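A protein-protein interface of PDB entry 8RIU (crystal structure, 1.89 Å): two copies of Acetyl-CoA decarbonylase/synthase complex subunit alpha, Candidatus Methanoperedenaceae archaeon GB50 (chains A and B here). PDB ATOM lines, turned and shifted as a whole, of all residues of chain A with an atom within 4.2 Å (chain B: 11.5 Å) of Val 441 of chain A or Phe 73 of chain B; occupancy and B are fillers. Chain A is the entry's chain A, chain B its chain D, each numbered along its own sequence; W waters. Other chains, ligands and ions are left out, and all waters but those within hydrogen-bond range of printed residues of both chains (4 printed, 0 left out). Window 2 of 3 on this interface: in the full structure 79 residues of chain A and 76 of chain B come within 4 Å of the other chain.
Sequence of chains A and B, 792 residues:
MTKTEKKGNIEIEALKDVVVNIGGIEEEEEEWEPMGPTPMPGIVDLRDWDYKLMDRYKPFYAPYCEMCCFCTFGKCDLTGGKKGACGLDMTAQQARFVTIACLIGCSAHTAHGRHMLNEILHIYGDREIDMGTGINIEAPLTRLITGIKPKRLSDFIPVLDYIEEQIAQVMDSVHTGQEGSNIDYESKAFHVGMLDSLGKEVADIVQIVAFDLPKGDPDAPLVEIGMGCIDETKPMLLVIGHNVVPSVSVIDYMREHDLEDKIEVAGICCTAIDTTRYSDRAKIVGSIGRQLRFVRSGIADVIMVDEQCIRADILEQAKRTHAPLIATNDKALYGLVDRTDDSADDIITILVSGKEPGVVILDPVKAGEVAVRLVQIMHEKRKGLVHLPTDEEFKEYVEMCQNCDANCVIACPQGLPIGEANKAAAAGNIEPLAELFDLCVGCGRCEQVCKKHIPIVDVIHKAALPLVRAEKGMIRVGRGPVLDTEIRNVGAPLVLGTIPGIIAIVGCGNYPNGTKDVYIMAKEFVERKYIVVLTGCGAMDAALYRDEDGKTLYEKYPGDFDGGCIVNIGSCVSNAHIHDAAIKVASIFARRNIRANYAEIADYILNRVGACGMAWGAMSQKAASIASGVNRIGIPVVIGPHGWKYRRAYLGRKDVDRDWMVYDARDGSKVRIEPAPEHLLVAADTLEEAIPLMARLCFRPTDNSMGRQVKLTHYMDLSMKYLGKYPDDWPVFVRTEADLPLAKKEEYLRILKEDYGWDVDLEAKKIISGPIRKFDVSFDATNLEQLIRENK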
ATOM      1  N   GLY A 289       5.835 -30.309 -14.628  1.00  0.00           N
ATOM      2  CA  GLY A 289       7.241 -29.908 -14.815  1.00  0.00           C
ATOM      3  C   GLY A 289       7.433 -28.997 -16.013  1.00  0.00           C
ATOM      4  O   GLY A 289       8.402 -28.229 -16.013  1.00  0.00           O
ATOM      5  N   PRO A 413      15.635 -28.297  -6.329  1.00  0.00           N
ATOM      6  CA  PRO A 413      15.234 -29.568  -5.707  1.00  0.00           C
ATOM      7  C   PRO A 413      15.974 -30.768  -6.271  1.00  0.00           C
ATOM      8  O   PRO A 413      16.118 -31.773  -5.564  1.00  0.00           O
ATOM      9  CB  PRO A 413      13.723 -29.645  -5.989  1.00  0.00           C
ATOM     10  CG  PRO A 413      13.504 -28.796  -7.188  1.00  0.00           C
ATOM     11  CD  PRO A 413      14.529 -27.684  -7.094  1.00  0.00           C
ATOM     12  N   GLN A 414      16.460 -30.695  -7.514  1.00  0.00           N
ATOM     13  CA  GLN A 414      17.204 -31.792  -8.124  1.00  0.00           C
ATOM     14  C   GLN A 414      18.715 -31.606  -8.061  1.00  0.00           C
ATOM     15  O   GLN A 414      19.449 -32.461  -8.567  1.00  0.00           O
ATOM     16  CB  GLN A 414      16.797 -31.983  -9.591  1.00  0.00           C
ATOM     17  CG  GLN A 414      15.324 -31.857  -9.871  1.00  0.00           C
ATOM     18  CD  GLN A 414      14.489 -32.761  -8.998  1.00  0.00           C
ATOM     19  OE1 GLN A 414      14.955 -33.805  -8.532  1.00  0.00           O
ATOM     20  NE2 GLN A 414      13.247 -32.362  -8.754  1.00  0.00           N
ATOM     21  N   LEU A 439      15.433 -32.650 -17.056  1.00  0.00           N
ATOM     22  CA  LEU A 439      15.641 -32.906 -15.634  1.00  0.00           C
ATOM     23  C   LEU A 439      14.982 -31.837 -14.774  1.00  0.00           C
ATOM     24  O   LEU A 439      14.567 -32.108 -13.637  1.00  0.00           O
ATOM     25  CB  LEU A 439      17.139 -32.965 -15.350  1.00  0.00           C
ATOM     26  CG  LEU A 439      17.923 -33.962 -16.200  1.00  0.00           C
ATOM     27  CD1 LEU A 439      19.367 -33.903 -15.797  1.00  0.00           C
ATOM     28  CD2 LEU A 439      17.378 -35.384 -16.049  1.00  0.00           C
ATOM     29  N   CYS A 440      14.883 -30.620 -15.300  1.00  0.00           N
ATOM     30  CA  CYS A 440      14.257 -29.515 -14.591  1.00  0.00           C
ATOM     31  C   CYS A 440      12.759 -29.750 -14.447  1.00  0.00           C
ATOM     32  O   CYS A 440      12.100 -30.224 -15.376  1.00  0.00           O
ATOM     33  CB  CYS A 440      14.522 -28.221 -15.362  1.00  0.00           C
ATOM     34  SG  CYS A 440      13.710 -26.752 -14.766  1.00  0.00           S
ATOM     35  N   VAL A 441      12.214 -29.412 -13.277  1.00  0.00           N
ATOM     36  CA  VAL A 441      10.783 -29.550 -13.021  1.00  0.00           C
ATOM     37  C   VAL A 441      10.093 -28.189 -12.977  1.00  0.00           C
ATOM     38  O   VAL A 441       8.998 -28.070 -12.427  1.00  0.00           O
ATOM     39  CB  VAL A 441      10.506 -30.354 -11.739  1.00  0.00           C
ATOM     40  CG1 VAL A 441      11.105 -31.754 -11.868  1.00  0.00           C
ATOM     41  CG2 VAL A 441      11.066 -29.638 -10.505  1.00  0.00           C
ATOM     42  N   GLY A 442      10.719 -27.163 -13.546  1.00  0.00           N
ATOM     43  CA  GLY A 442      10.051 -25.882 -13.741  1.00  0.00           C
ATOM     44  C   GLY A 442       9.528 -25.225 -12.482  1.00  0.00           C
ATOM     45  O   GLY A 442       8.412 -24.686 -12.489  1.00  0.00           O
ATOM     46  N   CYS A 443      10.321 -25.226 -11.407  1.00  0.00           N
ATOM     47  CA  CYS A 443       9.894 -24.663 -10.133  1.00  0.00           C
ATOM     48  C   CYS A 443      10.323 -23.211  -9.928  1.00  0.00           C
ATOM     49  O   CYS A 443       9.646 -22.478  -9.198  1.00  0.00           O
ATOM     50  CB  CYS A 443      10.433 -25.518  -8.980  1.00  0.00           C
ATOM     51  SG  CYS A 443      12.225 -25.358  -8.666  1.00  0.00           S
ATOM     52  N   ARG A 445      13.037 -22.001  -8.309  1.00  0.00           N
ATOM     53  CA  ARG A 445      13.707 -21.627  -7.035  1.00  0.00           C
ATOM     54  C   ARG A 445      15.138 -21.154  -7.324  1.00  0.00           C
ATOM     55  O   ARG A 445      15.574 -20.195  -6.690  1.00  0.00           O
ATOM     56  CB  ARG A 445      13.686 -22.807  -6.063  1.00  0.00           C
ATOM     57  CG  ARG A 445      12.331 -23.107  -5.441  1.00  0.00           C
ATOM     58  CD  ARG A 445      12.450 -23.670  -4.036  1.00  0.00           C
ATOM     59  NE  ARG A 445      13.410 -24.755  -3.921  1.00  0.00           N
ATOM     60  CZ  ARG A 445      13.108 -26.002  -3.588  1.00  0.00           C
ATOM     61  NH1 ARG A 445      11.876 -26.311  -3.230  1.00  0.00           N
ATOM     62  NH2 ARG A 445      14.038 -26.937  -3.614  1.00  0.00           N
ATOM     63  N   GLY A 509       4.957 -35.055 -11.598  1.00  0.00           N
ATOM     64  CA  GLY A 509       6.240 -35.103 -12.309  1.00  0.00           C
ATOM     65  C   GLY A 509       7.428 -34.569 -11.532  1.00  0.00           C
ATOM     66  O   GLY A 509       8.347 -34.064 -12.169  1.00  0.00           O
ATOM     67  N   ASN A 510       7.411 -34.680 -10.209  1.00  0.00           N
ATOM     68  CA  ASN A 510       8.621 -34.326  -9.460  1.00  0.00           C
ATOM     69  C   ASN A 510       9.571 -35.523  -9.474  1.00  0.00           C
ATOM     70  O   ASN A 510       9.852 -36.154  -8.451  1.00  0.00           O
ATOM     71  CB  ASN A 510       8.290 -33.907  -8.036  1.00  0.00           C
ATOM     72  CG  ASN A 510       9.525 -33.464  -7.259  1.00  0.00           C
ATOM     73  OD1 ASN A 510      10.543 -33.096  -7.848  1.00  0.00           O
ATOM     74  ND2 ASN A 510       9.448 -33.522  -5.933  1.00  0.00           N
ATOM     75  N   MET A 619       4.129 -35.833  -5.687  1.00  0.00           N
ATOM     76  CA  MET A 619       4.407 -34.483  -5.199  1.00  0.00           C
ATOM     77  C   MET A 619       3.267 -33.885  -4.376  1.00  0.00           C
ATOM     78  O   MET A 619       3.490 -33.419  -3.255  1.00  0.00           O
ATOM     79  CB  MET A 619       4.722 -33.585  -6.404  1.00  0.00           C
ATOM     80  CG  MET A 619       4.956 -32.087  -6.138  1.00  0.00           C
ATOM     81  SD  MET A 619       3.427 -31.156  -5.881  1.00  0.00           S
ATOM     82  CE  MET A 619       2.902 -30.897  -7.572  1.00  0.00           C
ATOM     83  N   MET B  67       9.596 -21.586   6.105  1.00  0.00           N
ATOM     84  CA  MET B  67       9.695 -22.668   5.104  1.00  0.00           C
ATOM     85  C   MET B  67       8.306 -23.224   4.778  1.00  0.00           C
ATOM     86  O   MET B  67       7.322 -22.723   5.325  1.00  0.00           O
ATOM     87  CB  MET B  67      10.578 -23.790   5.658  1.00  0.00           C
ATOM     88  CG  MET B  67      11.975 -23.346   6.045  1.00  0.00           C
ATOM     89  SD  MET B  67      12.909 -24.647   6.895  1.00  0.00           S
ATOM     90  CE  MET B  67      12.086 -24.662   8.484  1.00  0.00           C
ATOM     91  N   CYS B  68       8.249 -24.195   3.874  1.00  0.00           N
ATOM     92  CA  CYS B  68       6.975 -24.881   3.568  1.00  0.00           C
ATOM     93  C   CYS B  68       7.307 -26.359   3.378  1.00  0.00           C
ATOM     94  O   CYS B  68       8.259 -26.653   2.664  1.00  0.00           O
ATOM     95  CB  CYS B  68       6.252 -24.328   2.349  1.00  0.00           C
ATOM     96  SG  CYS B  68       4.652 -25.126   2.074  1.00  0.00           S
ATOM     97  N   CYS B  69       6.535 -27.229   4.013  1.00  0.00           N
ATOM     98  CA  CYS B  69       6.778 -28.664   3.984  1.00  0.00           C
ATOM     99  C   CYS B  69       5.660 -29.444   3.298  1.00  0.00           C
ATOM    100  O   CYS B  69       5.665 -30.678   3.358  1.00  0.00           O
ATOM    101  CB  CYS B  69       6.947 -29.188   5.414  1.00  0.00           C
ATOM    102  SG  CYS B  69       5.530 -28.851   6.448  1.00  0.00           S
ATOM    103  N   PHE B  70       4.707 -28.765   2.645  1.00  0.00           N
ATOM    104  CA  PHE B  70       3.435 -29.391   2.295  1.00  0.00           C
ATOM    105  C   PHE B  70       3.485 -30.304   1.068  1.00  0.00           C
ATOM    106  O   PHE B  70       2.512 -31.029   0.845  1.00  0.00           O
ATOM    107  CB  PHE B  70       2.357 -28.324   2.049  1.00  0.00           C
ATOM    108  CG  PHE B  70       2.051 -27.449   3.244  1.00  0.00           C
ATOM    109  CD1 PHE B  70       2.673 -27.641   4.468  1.00  0.00           C
ATOM    110  CD2 PHE B  70       1.112 -26.434   3.136  1.00  0.00           C
ATOM    111  CE1 PHE B  70       2.371 -26.830   5.556  1.00  0.00           C
ATOM    112  CE2 PHE B  70       0.808 -25.623   4.221  1.00  0.00           C
ATOM    113  CZ  PHE B  70       1.440 -25.823   5.430  1.00  0.00           C
ATOM    114  N   CYS B  71       4.562 -30.294   0.278  1.00  0.00           N
ATOM    115  CA  CYS B  71       4.629 -31.088  -0.948  1.00  0.00           C
ATOM    116  C   CYS B  71       6.083 -31.443  -1.239  1.00  0.00           C
ATOM    117  O   CYS B  71       7.004 -30.825  -0.705  1.00  0.00           O
ATOM    118  CB  CYS B  71       3.966 -30.334  -2.117  1.00  0.00           C
ATOM    119  SG  CYS B  71       5.063 -29.363  -3.198  1.00  0.00           S
ATOM    120  N   THR B  72       6.286 -32.466  -2.087  1.00  0.00           N
ATOM    121  CA  THR B  72       7.626 -33.025  -2.250  1.00  0.00           C
ATOM    122  C   THR B  72       8.552 -32.169  -3.112  1.00  0.00           C
ATOM    123  O   THR B  72       9.737 -32.500  -3.205  1.00  0.00           O
ATOM    124  CB  THR B  72       7.585 -34.448  -2.848  1.00  0.00           C
ATOM    125  OG1 THR B  72       7.317 -34.393  -4.258  1.00  0.00           O
ATOM    126  CG2 THR B  72       6.559 -35.307  -2.165  1.00  0.00           C
ATOM    127  N   PHE B  73       8.055 -31.104  -3.762  1.00  0.00           N
ATOM    128  CA  PHE B  73       8.967 -30.112  -4.332  1.00  0.00           C
ATOM    129  C   PHE B  73       9.801 -29.456  -3.239  1.00  0.00           C
ATOM    130  O   PHE B  73      10.951 -29.070  -3.485  1.00  0.00           O
ATOM    131  CB  PHE B  73       8.205 -29.006  -5.071  1.00  0.00           C
ATOM    132  CG  PHE B  73       7.692 -29.386  -6.425  1.00  0.00           C
ATOM    133  CD1 PHE B  73       8.434 -30.168  -7.290  1.00  0.00           C
ATOM    134  CD2 PHE B  73       6.437 -28.960  -6.833  1.00  0.00           C
ATOM    135  CE1 PHE B  73       7.945 -30.497  -8.536  1.00  0.00           C
ATOM    136  CE2 PHE B  73       5.939 -29.300  -8.082  1.00  0.00           C
ATOM    137  CZ  PHE B  73       6.691 -30.066  -8.928  1.00  0.00           C
ATOM    138  N   GLY B  74       9.237 -29.352  -2.041  1.00  0.00           N
ATOM    139  CA  GLY B  74       9.946 -28.713  -0.925  1.00  0.00           C
ATOM    140  C   GLY B  74      11.106 -29.559  -0.446  1.00  0.00           C
ATOM    141  O   GLY B  74      11.475 -30.494  -1.152  1.00  0.00           O
ATOM    142  N   LYS B  75      11.624 -29.261   0.743  1.00  0.00           N
ATOM    143  CA  LYS B  75      11.137 -28.155   1.606  1.00  0.00           C
ATOM    144  C   LYS B  75      11.549 -26.812   1.010  1.00  0.00           C
ATOM    145  O   LYS B  75      12.724 -26.635   0.718  1.00  0.00           O
ATOM    146  CB  LYS B  75      11.693 -28.287   3.023  1.00  0.00           C
ATOM    147  CG  LYS B  75      11.084 -27.355   4.062  1.00  0.00           C
ATOM    148  CD  LYS B  75      10.562 -28.070   5.290  1.00  0.00           C
ATOM    149  CE  LYS B  75      11.563 -29.014   5.919  1.00  0.00           C
ATOM    150  NZ  LYS B  75      12.599 -28.294   6.692  1.00  0.00           N
ATOM    151  N   CYS B  76      10.594 -25.905   0.876  1.00  0.00           N
ATOM    152  CA  CYS B  76      10.888 -24.623   0.205  1.00  0.00           C
ATOM    153  C   CYS B  76      11.286 -23.557   1.221  1.00  0.00           C
ATOM    154  O   CYS B  76      10.643 -23.460   2.259  1.00  0.00           O
ATOM    155  CB  CYS B  76       9.693 -24.123  -0.607  1.00  0.00           C
ATOM    156  SG  CYS B  76       9.332 -25.034  -2.126  1.00  0.00           S
ATOM    157  N   ASP B  77      12.369 -22.855   0.946  1.00  0.00           N
ATOM    158  CA  ASP B  77      12.755 -21.702   1.742  1.00  0.00           C
ATOM    159  C   ASP B  77      12.086 -20.466   1.156  1.00  0.00           C
ATOM    160  O   ASP B  77      12.304 -20.135  -0.017  1.00  0.00           O
ATOM    161  CB  ASP B  77      14.264 -21.505   1.783  1.00  0.00           C
ATOM    162  CG  ASP B  77      14.644 -20.241   2.513  1.00  0.00           C
ATOM    163  OD1 ASP B  77      13.987 -19.949   3.531  1.00  0.00           O
ATOM    164  OD2 ASP B  77      15.575 -19.535   2.075  1.00  0.00           O
ATOM    165  N   LEU B  78      11.293 -19.783   1.980  1.00  0.00           N
ATOM    166  CA  LEU B  78      10.546 -18.598   1.581  1.00  0.00           C
ATOM    167  C   LEU B  78      11.097 -17.327   2.211  1.00  0.00           C
ATOM    168  O   LEU B  78      10.480 -16.262   2.080  1.00  0.00           O
ATOM    169  CB  LEU B  78       9.073 -18.778   1.950  1.00  0.00           C
ATOM    170  CG  LEU B  78       8.428 -20.079   1.444  1.00  0.00           C
ATOM    171  CD1 LEU B  78       7.002 -20.197   1.933  1.00  0.00           C
ATOM    172  CD2 LEU B  78       8.454 -20.176  -0.077  1.00  0.00           C
ATOM    173  N   LYS B  83       9.529 -17.036  -3.441  1.00  0.00           N
ATOM    174  CA  LYS B  83       8.444 -17.886  -3.900  1.00  0.00           C
ATOM    175  C   LYS B  83       8.840 -19.348  -3.775  1.00  0.00           C
ATOM    176  O   LYS B  83       9.977 -19.725  -4.068  1.00  0.00           O
ATOM    177  CB  LYS B  83       8.092 -17.576  -5.352  1.00  0.00           C
ATOM    178  CG  LYS B  83       7.498 -16.202  -5.569  1.00  0.00           C
ATOM    179  CD  LYS B  83       6.989 -16.057  -6.992  1.00  0.00           C
ATOM    180  CE  LYS B  83       8.118 -15.914  -7.982  1.00  0.00           C
ATOM    181  NZ  LYS B  83       7.628 -15.798  -9.394  1.00  0.00           N
ATOM    182  N   GLY B  84       7.894 -20.168  -3.361  1.00  0.00           N
ATOM    183  CA  GLY B  84       8.136 -21.591  -3.308  1.00  0.00           C
ATOM    184  C   GLY B  84       8.213 -22.209  -4.691  1.00  0.00           C
ATOM    185  O   GLY B  84       7.964 -21.575  -5.721  1.00  0.00           O
ATOM    186  N   ALA B  85       8.562 -23.500  -4.698  1.00  0.00           N
ATOM    187  CA  ALA B  85       8.710 -24.238  -5.948  1.00  0.00           C
ATOM    188  C   ALA B  85       7.405 -24.308  -6.734  1.00  0.00           C
ATOM    189  O   ALA B  85       7.430 -24.636  -7.927  1.00  0.00           O
ATOM    190  CB  ALA B  85       9.239 -25.645  -5.645  1.00  0.00           C
ATOM    191  N   CYS B  86       6.272 -24.009  -6.099  1.00  0.00           N
ATOM    192  CA  CYS B  86       4.985 -23.919  -6.780  1.00  0.00           C
ATOM    193  C   CYS B  86       4.682 -22.511  -7.283  1.00  0.00           C
ATOM    194  O   CYS B  86       3.670 -22.318  -7.966  1.00  0.00           O
ATOM    195  CB  CYS B  86       3.866 -24.377  -5.842  1.00  0.00           C
ATOM    196  SG  CYS B  86       3.804 -23.453  -4.274  1.00  0.00           S
ATOM    197  N   GLY B  87       5.537 -21.531  -6.982  1.00  0.00           N
ATOM    198  CA  GLY B  87       5.293 -20.149  -7.339  1.00  0.00           C
ATOM    199  C   GLY B  87       4.631 -19.322  -6.255  1.00  0.00           C
ATOM    200  O   GLY B  87       4.489 -18.101  -6.429  1.00  0.00           O
ATOM    201  N   LEU B  88       4.223 -19.949  -5.148  1.00  0.00           N
ATOM    202  CA  LEU B  88       3.540 -19.239  -4.072  1.00  0.00           C
ATOM    203  C   LEU B  88       4.520 -18.380  -3.288  1.00  0.00           C
ATOM    204  O   LEU B  88       5.555 -18.864  -2.819  1.00  0.00           O
ATOM    205  CB  LEU B  88       2.857 -20.237  -3.135  1.00  0.00           C
ATOM    206  CG  LEU B  88       1.903 -19.633  -2.106  1.00  0.00           C
ATOM    207  CD1 LEU B  88       0.684 -19.070  -2.793  1.00  0.00           C
ATOM    208  CD2 LEU B  88       1.489 -20.661  -1.055  1.00  0.00           C
ATOM    209  N   ARG B  96      -2.125 -18.763   3.656  1.00  0.00           N
ATOM    210  CA  ARG B  96      -2.571 -20.143   3.479  1.00  0.00           C
ATOM    211  C   ARG B  96      -2.474 -20.912   4.786  1.00  0.00           C
ATOM    212  O   ARG B  96      -3.345 -21.731   5.102  1.00  0.00           O
ATOM    213  CB  ARG B  96      -1.753 -20.846   2.388  1.00  0.00           C
ATOM    214  CG  ARG B  96      -2.119 -22.321   2.232  1.00  0.00           C
ATOM    215  CD  ARG B  96      -1.646 -22.973   0.930  1.00  0.00           C
ATOM    216  NE  ARG B  96      -0.247 -23.357   0.993  1.00  0.00           N
ATOM    217  CZ  ARG B  96       0.321 -24.331   0.291  1.00  0.00           C
ATOM    218  NH1 ARG B  96      -0.394 -25.204  -0.400  1.00  0.00           N
ATOM    219  NH2 ARG B  96       1.644 -24.443   0.300  1.00  0.00           N
ATOM    220  N   HIS B 175      -4.669 -26.567  -1.387  1.00  0.00           N
ATOM    221  CA  HIS B 175      -3.845 -27.519  -2.168  1.00  0.00           C
ATOM    222  C   HIS B 175      -2.815 -26.729  -2.969  1.00  0.00           C
ATOM    223  O   HIS B 175      -3.046 -25.564  -3.315  1.00  0.00           O
ATOM    224  CB  HIS B 175      -4.691 -28.383  -3.103  1.00  0.00           C
ATOM    225  CG  HIS B 175      -3.956 -29.527  -3.714  1.00  0.00           C
ATOM    226  ND1 HIS B 175      -3.088 -29.377  -4.771  1.00  0.00           N
ATOM    227  CD2 HIS B 175      -3.955 -30.829  -3.422  1.00  0.00           C
ATOM    228  CE1 HIS B 175      -2.585 -30.555  -5.091  1.00  0.00           C
ATOM    229  NE2 HIS B 175      -3.098 -31.451  -4.285  1.00  0.00           N
ATOM    230  N   THR B 176      -1.688 -27.365  -3.234  1.00  0.00           N
ATOM    231  CA  THR B 176      -0.643 -26.736  -4.023  1.00  0.00           C
ATOM    232  C   THR B 176      -1.187 -26.308  -5.379  1.00  0.00           C
ATOM    233  O   THR B 176      -1.971 -27.021  -6.012  1.00  0.00           O
ATOM    234  CB  THR B 176       0.524 -27.708  -4.189  1.00  0.00           C
ATOM    235  OG1 THR B 176       1.041 -28.048  -2.893  1.00  0.00           O
ATOM    236  CG2 THR B 176       1.628 -27.101  -5.036  1.00  0.00           C
ATOM    237  N   GLY B 177      -0.774 -25.126  -5.820  1.00  0.00           N
ATOM    238  CA  GLY B 177      -1.167 -24.651  -7.135  1.00  0.00           C
ATOM    239  C   GLY B 177      -2.577 -24.110  -7.183  1.00  0.00           C
ATOM    240  O   GLY B 177      -3.303 -24.355  -8.162  1.00  0.00           O
ATOM    241  N   GLN B 178      -2.991 -23.385  -6.144  1.00  0.00           N
ATOM    242  CA  GLN B 178      -4.312 -22.775  -6.079  1.00  0.00           C
ATOM    243  C   GLN B 178      -4.161 -21.263  -5.922  1.00  0.00           C
ATOM    244  O   GLN B 178      -3.445 -20.629  -6.706  1.00  0.00           O
ATOM    245  CB  GLN B 178      -5.117 -23.399  -4.937  1.00  0.00           C
ATOM    246  CG  GLN B 178      -5.487 -24.853  -5.183  1.00  0.00           C
ATOM    247  CD  GLN B 178      -6.728 -25.019  -6.040  1.00  0.00           C
ATOM    248  OE1 GLN B 178      -6.826 -24.473  -7.140  1.00  0.00           O
ATOM    249  NE2 GLN B 178      -7.681 -25.800  -5.543  1.00  0.00           N
HETATM  250  O   HOH W   1      14.313 -23.497  -1.034  1.00  0.00           O
HETATM  251  O   HOH W   2      13.961 -29.453  -2.056  1.00  0.00           O
HETATM  252  O   HOH W   3      15.308 -26.132  -0.557  1.00  0.00           O
HETATM  253  O   HOH W   4      10.081 -20.418  -7.535  1.00  0.00           O
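The side-chain hydroxyl (OG1) of Thr 72 of chain B sits at hydrogen-bond distance from the side-chain amide nitrogen (ND2) of Asn 510 of chain A.
O of Phe 73 of chain B lies within hydrogen-bond range of NH1 of Arg 445 of chain A.
NH1 of Arg 445 of chain A lies close to SG of Cys 76 of chain B (3.1 Å).
The side-chain sulfur of Cys 71 of chain B sits close to the side-chain sulfur of Met 619 of chain A.
O of Ala 85 of chain B sits close to O of Cys 443 of chain A, 3.3 Å away.
The backbone carbonyl oxygen of Met 619 of chain A sits at hydrogen-bond distance from the backbone NH of Thr 72 of chain B.
The backbone NH of Cys 68 of chain B is in hydrogen-bond range of the backbone carbonyl oxygen of Cys 76 of chain B (3.0 Å).
NE2 of Gln 414 of chain A is in hydrogen-bond range of OD1 of Asn 510 of chain A (2.9 Å).
The side-chain sulfur of Cys 71 of chain B sits close to the backbone NH of Phe 73 of chain B (3.5 Å).
SG of Cys 76 of chain B lies close to N of Ala 85 of chain B, at 3.1 Å.
The side-chain sulfur (SG) of Cys 443 of chain A sits close to the backbone NH (N) of Arg 445 of chain A (3.5 Å).
Pro 413 of chain A touches Phe 73 of chain B.
CE1 of Phe 73 of chain B touches CG2 of Val 441 of chain A, at 3.8 Å.
O of Gly 84 of chain B touches O of Cys 443 of chain A (3.97 Å).
CA of Gly 74 of chain B touches NH1 of Arg 445 of chain A (3.8 Å).
Ala 85 of chain B touches Arg 445 of chain A (CB to NH1, 3.6 Å).
Phe 73 of chain B touches Asn 510 of chain A (CE1 to CB, 3.5 Å).
Met 619 of chain A touches Phe 73 of chain B (CE to CE2, 3.5 Å).
Val 441 of chain A touches just one residue of chain B: Phe 73.
Phe 73 of chain B touches just these residues of chain A: Pro 413, Val 441, Arg 445, Asn 510 and Met 619.
No residue of chain B comes within 4 Å of Gly 289 of chain A.
Of chain B, only Phe 73 (3.8 Å) comes within 4 Å of Pro 413 of chain A.
No residue of chain B comes within 4 Å of Cys 440 of chain A.
Cys 443 of chain A touches two residues of chain B.
No residue of chain B comes within 4 Å of Gly 509 of chain A.
Asn 510 of chain A touches just these residues of chain B: Thr 72 (2.8 Å) and Phe 73 (3.5 Å).
Of the printed residues of chain B, Met 619 of chain A touches Cys 71 (3.3 Å), Thr 72 (3.1 Å) and Phe 73 (3.5 Å).
Of the printed residues of chain A, Cys 71 of chain B touches Met 619 (3.3 Å).
Printed residues of chain A within 4 Å of Gly 74 of chain B: Arg 445 (3.8 Å).
Printed residues of chain B within 4 Å of Arg 445 of chain A: Phe 73, Gly 74, Cys 76 and Ala 85.
Printed residues of chain A within 4 Å of Gly 84 of chain B: Cys 443 (3.97 Å).
Met 67 of chain B touches none of the printed residues of chain A.
The nearest printed residue of chain A that does not touch Phe 73 of chain B is Gly 509 of chain A (5.1 Å).
Printed residues of chain A that touch a printed residue of chain B: Pro 413, Val 441, Cys 443, Arg 445, Asn 510 and Met 619.
Hydrophobic or aromatic side chains of chain A that line the printed part of chain B: Pro 413, Val 441 and Met 619.
Of the 23 printed residues of chain B, 7 touch a printed residue of chain A.
Among the printed residues, 13 pairs touch across the chains.
No position is printed for both chains.
Of the 13 pairs that touch across the chains among the printed residues, none has its exchanged pair printed and touching as well.
Water W4 lies within hydrogen-bond range of O of Cys 443 of chain A (2.7 Å), O of Gly 84 of chain B (3.0 Å) and N of Arg 445 of chain A (3.4 Å).
Water W2 lies within hydrogen-bond range of the backbone carbonyl oxygen of Gly 74 of chain B (2.8 Å), the guanidinium group of Arg 445 of chain A (3.0 Å) and the backbone carbonyl oxygen of Phe 73 of chain B (3.4 Å).
Water W1 lies within hydrogen-bond range of N of Asp 77 of chain B and NE of Arg 445 of chain A.
Water W3 bridges the backbone carbonyl oxygen of Lys 75 of chain B (2.9 Å) and the guanidinium group of Arg 445 of chain A (3.4 Å).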
